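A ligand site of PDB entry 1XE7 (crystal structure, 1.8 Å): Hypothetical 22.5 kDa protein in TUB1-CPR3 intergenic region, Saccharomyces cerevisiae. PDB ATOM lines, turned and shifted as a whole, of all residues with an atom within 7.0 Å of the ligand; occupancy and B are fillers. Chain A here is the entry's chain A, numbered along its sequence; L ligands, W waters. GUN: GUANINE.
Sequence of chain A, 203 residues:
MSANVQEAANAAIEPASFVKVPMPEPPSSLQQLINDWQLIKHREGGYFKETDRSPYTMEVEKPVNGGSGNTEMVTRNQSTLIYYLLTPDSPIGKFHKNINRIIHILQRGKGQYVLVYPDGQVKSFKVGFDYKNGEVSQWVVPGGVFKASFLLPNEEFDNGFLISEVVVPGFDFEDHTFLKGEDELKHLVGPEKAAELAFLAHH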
ATOM      1  N   ILE A  40     -23.061  -8.792   3.576  1.00  0.00           N
ATOM      2  CA  ILE A  40     -22.794  -7.414   3.956  1.00  0.00           C
ATOM      3  C   ILE A  40     -23.820  -6.495   3.311  1.00  0.00           C
ATOM      4  O   ILE A  40     -24.429  -6.848   2.309  1.00  0.00           O
ATOM      5  CB  ILE A  40     -21.381  -6.974   3.514  1.00  0.00           C
ATOM      6  CG1 ILE A  40     -21.279  -7.000   1.986  1.00  0.00           C
ATOM      7  CG2 ILE A  40     -20.334  -7.895   4.129  1.00  0.00           C
ATOM      8  CD1 ILE A  40     -19.971  -6.481   1.441  1.00  0.00           C
ATOM      9  N   HIS A  42     -25.344  -3.879   0.995  1.00  0.00           N
ATOM     10  CA  HIS A  42     -25.015  -3.357  -0.335  1.00  0.00           C
ATOM     11  C   HIS A  42     -25.268  -1.851  -0.347  1.00  0.00           C
ATOM     12  O   HIS A  42     -26.125  -1.359   0.392  1.00  0.00           O
ATOM     13  CB  HIS A  42     -25.887  -4.052  -1.394  1.00  0.00           C
ATOM     14  CG  HIS A  42     -25.487  -3.752  -2.804  1.00  0.00           C
ATOM     15  ND1 HIS A  42     -25.708  -2.523  -3.389  1.00  0.00           N
ATOM     16  CD2 HIS A  42     -24.855  -4.508  -3.727  1.00  0.00           C
ATOM     17  CE1 HIS A  42     -25.224  -2.542  -4.619  1.00  0.00           C
ATOM     18  NE2 HIS A  42     -24.698  -3.731  -4.851  1.00  0.00           N
ATOM     19  N   ARG A  43     -24.534  -1.127  -1.176  1.00  0.00           N
ATOM     20  CA  ARG A  43     -24.671   0.332  -1.254  1.00  0.00           C
ATOM     21  C   ARG A  43     -26.075   0.768  -1.661  1.00  0.00           C
ATOM     22  O   ARG A  43     -26.519   1.861  -1.306  1.00  0.00           O
ATOM     23  CB  ARG A  43     -23.677   0.918  -2.263  1.00  0.00           C
ATOM     24  CG  ARG A  43     -22.235   0.471  -2.065  1.00  0.00           C
ATOM     25  CD  ARG A  43     -21.338   1.063  -3.148  1.00  0.00           C
ATOM     26  NE  ARG A  43     -20.093   0.299  -3.303  1.00  0.00           N
ATOM     27  CZ  ARG A  43     -19.080   0.675  -4.084  1.00  0.00           C
ATOM     28  NH1 ARG A  43     -19.160   1.804  -4.774  1.00  0.00           N
ATOM     29  NH2 ARG A  43     -17.997  -0.076  -4.175  1.00  0.00           N
ATOM     30  N   GLU A  44     -26.770  -0.072  -2.413  1.00  0.00           N
ATOM     31  CA  GLU A  44     -28.118   0.255  -2.870  1.00  0.00           C
ATOM     32  C   GLU A  44     -29.219  -0.263  -1.944  1.00  0.00           C
ATOM     33  O   GLU A  44     -30.394  -0.077  -2.224  1.00  0.00           O
ATOM     34  CB  GLU A  44     -28.346  -0.300  -4.278  1.00  0.00           C
ATOM     35  CG  GLU A  44     -27.987   0.669  -5.401  1.00  0.00           C
ATOM     36  CD  GLU A  44     -26.572   1.199  -5.311  1.00  0.00           C
ATOM     37  OE1 GLU A  44     -26.347   2.151  -4.538  1.00  0.00           O
ATOM     38  OE2 GLU A  44     -25.696   0.653  -5.990  1.00  0.00           O
ATOM     39  N   PHE A  48     -25.809  -8.699   0.672  1.00  0.00           N
ATOM     40  CA  PHE A  48     -25.297  -9.494  -0.437  1.00  0.00           C
ATOM     41  C   PHE A  48     -23.904 -10.046  -0.202  1.00  0.00           C
ATOM     42  O   PHE A  48     -23.232  -9.692   0.764  1.00  0.00           O
ATOM     43  CB  PHE A  48     -25.252  -8.626  -1.695  1.00  0.00           C
ATOM     44  CG  PHE A  48     -23.962  -7.859  -1.858  1.00  0.00           C
ATOM     45  CD1 PHE A  48     -23.012  -8.260  -2.802  1.00  0.00           C
ATOM     46  CD2 PHE A  48     -23.678  -6.775  -1.041  1.00  0.00           C
ATOM     47  CE1 PHE A  48     -21.799  -7.583  -2.919  1.00  0.00           C
ATOM     48  CE2 PHE A  48     -22.464  -6.089  -1.148  1.00  0.00           C
ATOM     49  CZ  PHE A  48     -21.515  -6.499  -2.092  1.00  0.00           C
ATOM     50  N   LYS A  49     -23.492 -10.911  -1.115  1.00  0.00           N
ATOM     51  CA  LYS A  49     -22.151 -11.471  -1.083  1.00  0.00           C
ATOM     52  C   LYS A  49     -21.835 -12.090  -2.428  1.00  0.00           C
ATOM     53  O   LYS A  49     -22.649 -12.803  -3.014  1.00  0.00           O
ATOM     54  CB  LYS A  49     -21.988 -12.549  -0.008  1.00  0.00           C
ATOM     55  CG  LYS A  49     -20.549 -13.044   0.059  1.00  0.00           C
ATOM     56  CD  LYS A  49     -20.261 -13.932   1.272  1.00  0.00           C
ATOM     57  CE  LYS A  49     -20.843 -15.327   1.108  1.00  0.00           C
ATOM     58  NZ  LYS A  49     -20.311 -16.248   2.161  1.00  0.00           N
ATOM     59  N   GLU A  50     -20.653 -11.785  -2.932  1.00  0.00           N
ATOM     60  CA  GLU A  50     -20.219 -12.343  -4.202  1.00  0.00           C
ATOM     61  C   GLU A  50     -19.665 -13.710  -3.834  1.00  0.00           C
ATOM     62  O   GLU A  50     -18.722 -13.809  -3.033  1.00  0.00           O
ATOM     63  CB  GLU A  50     -19.155 -11.461  -4.844  1.00  0.00           C
ATOM     64  CG  GLU A  50     -18.605 -12.005  -6.158  1.00  0.00           C
ATOM     65  CD  GLU A  50     -17.602 -11.064  -6.802  1.00  0.00           C
ATOM     66  OE1 GLU A  50     -18.028 -10.036  -7.358  1.00  0.00           O
ATOM     67  OE2 GLU A  50     -16.385 -11.362  -6.741  1.00  0.00           O
ATOM     68  N   THR A  51     -20.269 -14.760  -4.385  1.00  0.00           N
ATOM     69  CA  THR A  51     -19.864 -16.123  -4.084  1.00  0.00           C
ATOM     70  C   THR A  51     -19.056 -16.771  -5.208  1.00  0.00           C
ATOM     71  O   THR A  51     -18.490 -17.853  -5.036  1.00  0.00           O
ATOM     72  CB  THR A  51     -21.086 -17.004  -3.780  1.00  0.00           C
ATOM     73  OG1 THR A  51     -22.018 -16.911  -4.871  1.00  0.00           O
ATOM     74  CG2 THR A  51     -21.776 -16.529  -2.503  1.00  0.00           C
ATOM     75  N   ASP A  52     -19.040 -16.134  -6.370  1.00  0.00           N
ATOM     76  CA  ASP A  52     -18.262 -16.656  -7.494  1.00  0.00           C
ATOM     77  C   ASP A  52     -17.869 -15.554  -8.453  1.00  0.00           C
ATOM     78  O   ASP A  52     -18.624 -14.604  -8.695  1.00  0.00           O
ATOM     79  CB  ASP A  52     -19.040 -17.767  -8.233  1.00  0.00           C
ATOM     80  CG  ASP A  52     -18.222 -18.416  -9.346  1.00  0.00           C
ATOM     81  OD1 ASP A  52     -18.359 -17.988 -10.518  1.00  0.00           O
ATOM     82  OD2 ASP A  52     -17.425 -19.344  -9.062  1.00  0.00           O
ATOM     83  N   ARG A  53     -16.649 -15.660  -8.961  1.00  0.00           N
ATOM     84  CA  ARG A  53     -16.099 -14.723  -9.925  1.00  0.00           C
ATOM     85  C   ARG A  53     -15.209 -15.622 -10.768  1.00  0.00           C
ATOM     86  O   ARG A  53     -14.209 -16.159 -10.280  1.00  0.00           O
ATOM     87  CB  ARG A  53     -15.282 -13.628  -9.224  1.00  0.00           C
ATOM     88  CG  ARG A  53     -14.705 -12.584 -10.186  1.00  0.00           C
ATOM     89  CD  ARG A  53     -14.058 -11.402  -9.461  1.00  0.00           C
ATOM     90  NE  ARG A  53     -15.015 -10.394  -9.021  1.00  0.00           N
ATOM     91  CZ  ARG A  53     -15.523  -9.431  -9.792  1.00  0.00           C
ATOM     92  NH1 ARG A  53     -16.393  -8.559  -9.279  1.00  0.00           N
ATOM     93  NH2 ARG A  53     -15.158  -9.320 -11.065  1.00  0.00           N
ATOM     94  N   THR A  80     -19.811 -13.150 -12.663  1.00  0.00           N
ATOM     95  CA  THR A  80     -19.823 -13.024 -11.220  1.00  0.00           C
ATOM     96  C   THR A  80     -21.217 -13.468 -10.757  1.00  0.00           C
ATOM     97  O   THR A  80     -22.208 -13.332 -11.490  1.00  0.00           O
ATOM     98  CB  THR A  80     -19.545 -11.600 -10.699  1.00  0.00           C
ATOM     99  OG1 THR A  80     -20.438 -10.662 -11.307  1.00  0.00           O
ATOM    100  CG2 THR A  80     -18.103 -11.198 -11.010  1.00  0.00           C
ATOM    101  N   LEU A  81     -21.270 -13.999  -9.545  1.00  0.00           N
ATOM    102  CA  LEU A  81     -22.495 -14.491  -8.955  1.00  0.00           C
ATOM    103  C   LEU A  81     -22.634 -13.951  -7.533  1.00  0.00           C
ATOM    104  O   LEU A  81     -21.664 -13.953  -6.779  1.00  0.00           O
ATOM    105  CB  LEU A  81     -22.459 -16.016  -8.893  1.00  0.00           C
ATOM    106  CG  LEU A  81     -23.451 -16.752  -7.986  1.00  0.00           C
ATOM    107  CD1 LEU A  81     -24.855 -16.626  -8.567  1.00  0.00           C
ATOM    108  CD2 LEU A  81     -23.065 -18.220  -7.867  1.00  0.00           C
ATOM    109  N   ILE A  82     -23.831 -13.472  -7.180  1.00  0.00           N
ATOM    110  CA  ILE A  82     -24.047 -12.990  -5.822  1.00  0.00           C
ATOM    111  C   ILE A  82     -25.374 -13.495  -5.267  1.00  0.00           C
ATOM    112  O   ILE A  82     -26.261 -13.932  -6.002  1.00  0.00           O
ATOM    113  CB  ILE A  82     -24.115 -11.433  -5.725  1.00  0.00           C
ATOM    114  CG1 ILE A  82     -25.371 -10.912  -6.455  1.00  0.00           C
ATOM    115  CG2 ILE A  82     -22.860 -10.804  -6.301  1.00  0.00           C
ATOM    116  CD1 ILE A  82     -25.685  -9.453  -6.180  1.00  0.00           C
ATOM    117  N   HIS A  96     -30.630   1.696  -9.780  1.00  0.00           N
ATOM    118  CA  HIS A  96     -29.263   1.679 -10.310  1.00  0.00           C
ATOM    119  C   HIS A  96     -29.290   0.889 -11.603  1.00  0.00           C
ATOM    120  O   HIS A  96     -30.217   0.125 -11.854  1.00  0.00           O
ATOM    121  CB  HIS A  96     -28.295   1.006  -9.325  1.00  0.00           C
ATOM    122  CG  HIS A  96     -28.528  -0.460  -9.164  1.00  0.00           C
ATOM    123  ND1 HIS A  96     -29.588  -0.969  -8.447  1.00  0.00           N
ATOM    124  CD2 HIS A  96     -27.862  -1.533  -9.658  1.00  0.00           C
ATOM    125  CE1 HIS A  96     -29.567  -2.296  -8.513  1.00  0.00           C
ATOM    126  NE2 HIS A  96     -28.528  -2.654  -9.242  1.00  0.00           N
ATOM    127  N   ASN A  98     -26.653  -1.152 -14.805  1.00  0.00           N
ATOM    128  CA  ASN A  98     -25.355  -1.698 -15.155  1.00  0.00           C
ATOM    129  C   ASN A  98     -25.324  -1.723 -16.676  1.00  0.00           C
ATOM    130  O   ASN A  98     -26.364  -1.875 -17.314  1.00  0.00           O
ATOM    131  CB  ASN A  98     -25.193  -3.130 -14.616  1.00  0.00           C
ATOM    132  CG  ASN A  98     -23.769  -3.649 -14.739  1.00  0.00           C
ATOM    133  OD1 ASN A  98     -23.223  -3.761 -15.847  1.00  0.00           O
ATOM    134  ND2 ASN A  98     -23.156  -3.957 -13.605  1.00  0.00           N
ATOM    135  N   GLU A 165     -27.935 -13.567  -8.425  1.00  0.00           N
ATOM    136  CA  GLU A 165     -27.801 -12.775  -9.640  1.00  0.00           C
ATOM    137  C   GLU A 165     -26.502 -13.142 -10.338  1.00  0.00           C
ATOM    138  O   GLU A 165     -25.468 -13.353  -9.694  1.00  0.00           O
ATOM    139  CB  GLU A 165     -27.787 -11.276  -9.310  1.00  0.00           C
ATOM    140  CG  GLU A 165     -29.118 -10.707  -8.811  1.00  0.00           C
ATOM    141  CD  GLU A 165     -29.007  -9.233  -8.467  1.00  0.00           C
ATOM    142  OE1 GLU A 165     -28.479  -8.468  -9.294  1.00  0.00           O
ATOM    143  OE2 GLU A 165     -29.448  -8.833  -7.370  1.00  0.00           O
ATOM    144  N   VAL A 167     -24.010 -11.861 -13.564  1.00  0.00           N
ATOM    145  CA  VAL A 167     -23.781 -10.845 -14.572  1.00  0.00           C
ATOM    146  C   VAL A 167     -22.614 -11.269 -15.446  1.00  0.00           C
ATOM    147  O   VAL A 167     -21.599 -11.778 -14.957  1.00  0.00           O
ATOM    148  CB  VAL A 167     -23.490  -9.445 -13.940  1.00  0.00           C
ATOM    149  CG1 VAL A 167     -22.162  -9.439 -13.240  1.00  0.00           C
ATOM    150  CG2 VAL A 167     -23.521  -8.366 -15.029  1.00  0.00           C
ATOM    151  N   GLY A 170     -18.471 -10.215 -15.939  1.00  0.00           N
ATOM    152  CA  GLY A 170     -18.511 -10.075 -14.488  1.00  0.00           C
ATOM    153  C   GLY A 170     -18.546  -8.643 -13.960  1.00  0.00           C
ATOM    154  O   GLY A 170     -17.992  -7.714 -14.564  1.00  0.00           O
ATOM    155  N   PHE A 171     -19.168  -8.480 -12.795  1.00  0.00           N
ATOM    156  CA  PHE A 171     -19.306  -7.166 -12.173  1.00  0.00           C
ATOM    157  C   PHE A 171     -18.018  -6.376 -11.956  1.00  0.00           C
ATOM    158  O   PHE A 171     -17.004  -6.904 -11.517  1.00  0.00           O
ATOM    159  CB  PHE A 171     -20.018  -7.275 -10.825  1.00  0.00           C
ATOM    160  CG  PHE A 171     -20.179  -5.959 -10.114  1.00  0.00           C
ATOM    161  CD1 PHE A 171     -21.279  -5.148 -10.373  1.00  0.00           C
ATOM    162  CD2 PHE A 171     -19.192  -5.490  -9.243  1.00  0.00           C
ATOM    163  CE1 PHE A 171     -21.405  -3.896  -9.782  1.00  0.00           C
ATOM    164  CE2 PHE A 171     -19.309  -4.240  -8.642  1.00  0.00           C
ATOM    165  CZ  PHE A 171     -20.419  -3.437  -8.921  1.00  0.00           C
ATOM    166  N   ASP A 172     -18.110  -5.081 -12.253  1.00  0.00           N
ATOM    167  CA  ASP A 172     -17.022  -4.138 -12.053  1.00  0.00           C
ATOM    168  C   ASP A 172     -17.734  -2.821 -11.727  1.00  0.00           C
ATOM    169  O   ASP A 172     -18.716  -2.476 -12.387  1.00  0.00           O
ATOM    170  CB  ASP A 172     -16.183  -3.978 -13.335  1.00  0.00           C
ATOM    171  CG  ASP A 172     -14.907  -3.187 -13.098  1.00  0.00           C
ATOM    172  OD1 ASP A 172     -14.987  -1.977 -12.785  1.00  0.00           O
ATOM    173  OD2 ASP A 172     -13.817  -3.776 -13.237  1.00  0.00           O
ATOM    174  N   PHE A 173     -17.263  -2.114 -10.716  1.00  0.00           N
ATOM    175  CA  PHE A 173     -17.918  -0.868 -10.329  1.00  0.00           C
ATOM    176  C   PHE A 173     -17.957   0.142 -11.469  1.00  0.00           C
ATOM    177  O   PHE A 173     -18.844   1.008 -11.527  1.00  0.00           O
ATOM    178  CB  PHE A 173     -17.224  -0.239  -9.119  1.00  0.00           C
ATOM    179  CG  PHE A 173     -17.997   0.899  -8.498  1.00  0.00           C
ATOM    180  CD1 PHE A 173     -17.352   2.089  -8.153  1.00  0.00           C
ATOM    181  CD2 PHE A 173     -19.362   0.780  -8.270  1.00  0.00           C
ATOM    182  CE1 PHE A 173     -18.074   3.150  -7.591  1.00  0.00           C
ATOM    183  CE2 PHE A 173     -20.085   1.831  -7.708  1.00  0.00           C
ATOM    184  CZ  PHE A 173     -19.440   3.021  -7.373  1.00  0.00           C
ATOM    185  N   HIS A 176     -21.216   0.148 -13.165  1.00  0.00           N
ATOM    186  CA  HIS A 176     -22.346   0.416 -12.281  1.00  0.00           C
ATOM    187  C   HIS A 176     -22.678   1.911 -12.157  1.00  0.00           C
ATOM    188  O   HIS A 176     -21.776   2.741 -12.026  1.00  0.00           O
ATOM    189  CB  HIS A 176     -22.016  -0.148 -10.892  1.00  0.00           C
ATOM    190  CG  HIS A 176     -23.122  -0.018  -9.899  1.00  0.00           C
ATOM    191  ND1 HIS A 176     -24.069  -0.990  -9.713  1.00  0.00           N
ATOM    192  CD2 HIS A 176     -23.403   0.968  -9.007  1.00  0.00           C
ATOM    193  CE1 HIS A 176     -24.895  -0.630  -8.744  1.00  0.00           C
ATOM    194  NE2 HIS A 176     -24.519   0.559  -8.302  1.00  0.00           N
HETATM  195  N9  GUN L   1     -19.261  -5.115  -4.607  1.00  0.00           N
HETATM  196  C8  GUN L   1     -19.980  -3.989  -4.324  1.00  0.00           C
HETATM  197  N7  GUN L   1     -21.137  -3.911  -4.945  1.00  0.00           N
HETATM  198  C5  GUN L   1     -21.183  -5.073  -5.693  1.00  0.00           C
HETATM  199  C6  GUN L   1     -22.203  -5.567  -6.595  1.00  0.00           C
HETATM  200  O6  GUN L   1     -23.275  -5.052  -6.907  1.00  0.00           O
HETATM  201  N1  GUN L   1     -21.835  -6.816  -7.156  1.00  0.00           N
HETATM  202  C2  GUN L   1     -20.645  -7.499  -6.891  1.00  0.00           C
HETATM  203  N2  GUN L   1     -20.464  -8.668  -7.509  1.00  0.00           N
HETATM  204  N3  GUN L   1     -19.697  -7.034  -6.052  1.00  0.00           N
HETATM  205  C4  GUN L   1     -20.030  -5.820  -5.491  1.00  0.00           C
HETATM  206  O   HOH W   1     -16.860  -7.136  -6.478  1.00  0.00           O
HETATM  207  O   HOH W   2     -22.366  -2.301  -2.596  1.00  0.00           O
HETATM  208  O   HOH W   3     -24.984  -5.770  -9.094  1.00  0.00           O
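Water W1 lies within hydrogen-bond range of N3 of the ligand, NH1 of Arg 53 and OE1 of Glu 50.
Water W2 lies within hydrogen-bond range of the backbone NH of Arg 43, a nitrogen (N7) of the ligand and a ring nitrogen (ND1) of His 42.
N2 of the ligand lies within hydrogen-bond range of OE1 of Glu 50 (2.8 Å).
An oxygen (O6) of the ligand is in hydrogen-bond range of a ring nitrogen (NE2) of His 42.
The side-chain carboxylate of Glu 50 is in salt-bridge range of the guanidinium group of Arg 53 (2.8 Å).
ND1 of His 42 lies within hydrogen-bond range of N of Glu 44, 2.8 Å away.
The backbone NH (N) of Phe 171 is in hydrogen-bond range of the side-chain hydroxyl (OG1) of Thr 80.
The backbone carbonyl oxygen of Phe 171 sits at hydrogen-bond distance from the guanidinium group of Arg 53 (2.8 Å).
The backbone carbonyl oxygen of Ile 82 is in hydrogen-bond range of the backbone NH of Glu 165 (3.0 Å).
O of Ile 40 lies within hydrogen-bond range of N of Phe 48, at 2.8 Å.
Residues that only touch the ligand: Phe 171, Ile 82 and Phe 48.
Hydrophobic or aromatic side chains that line the ligand: His 42, Phe 48, Ile 82 and Phe 171.
Of the 22 residues printed, 5 come within 4 Å of the ligand.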
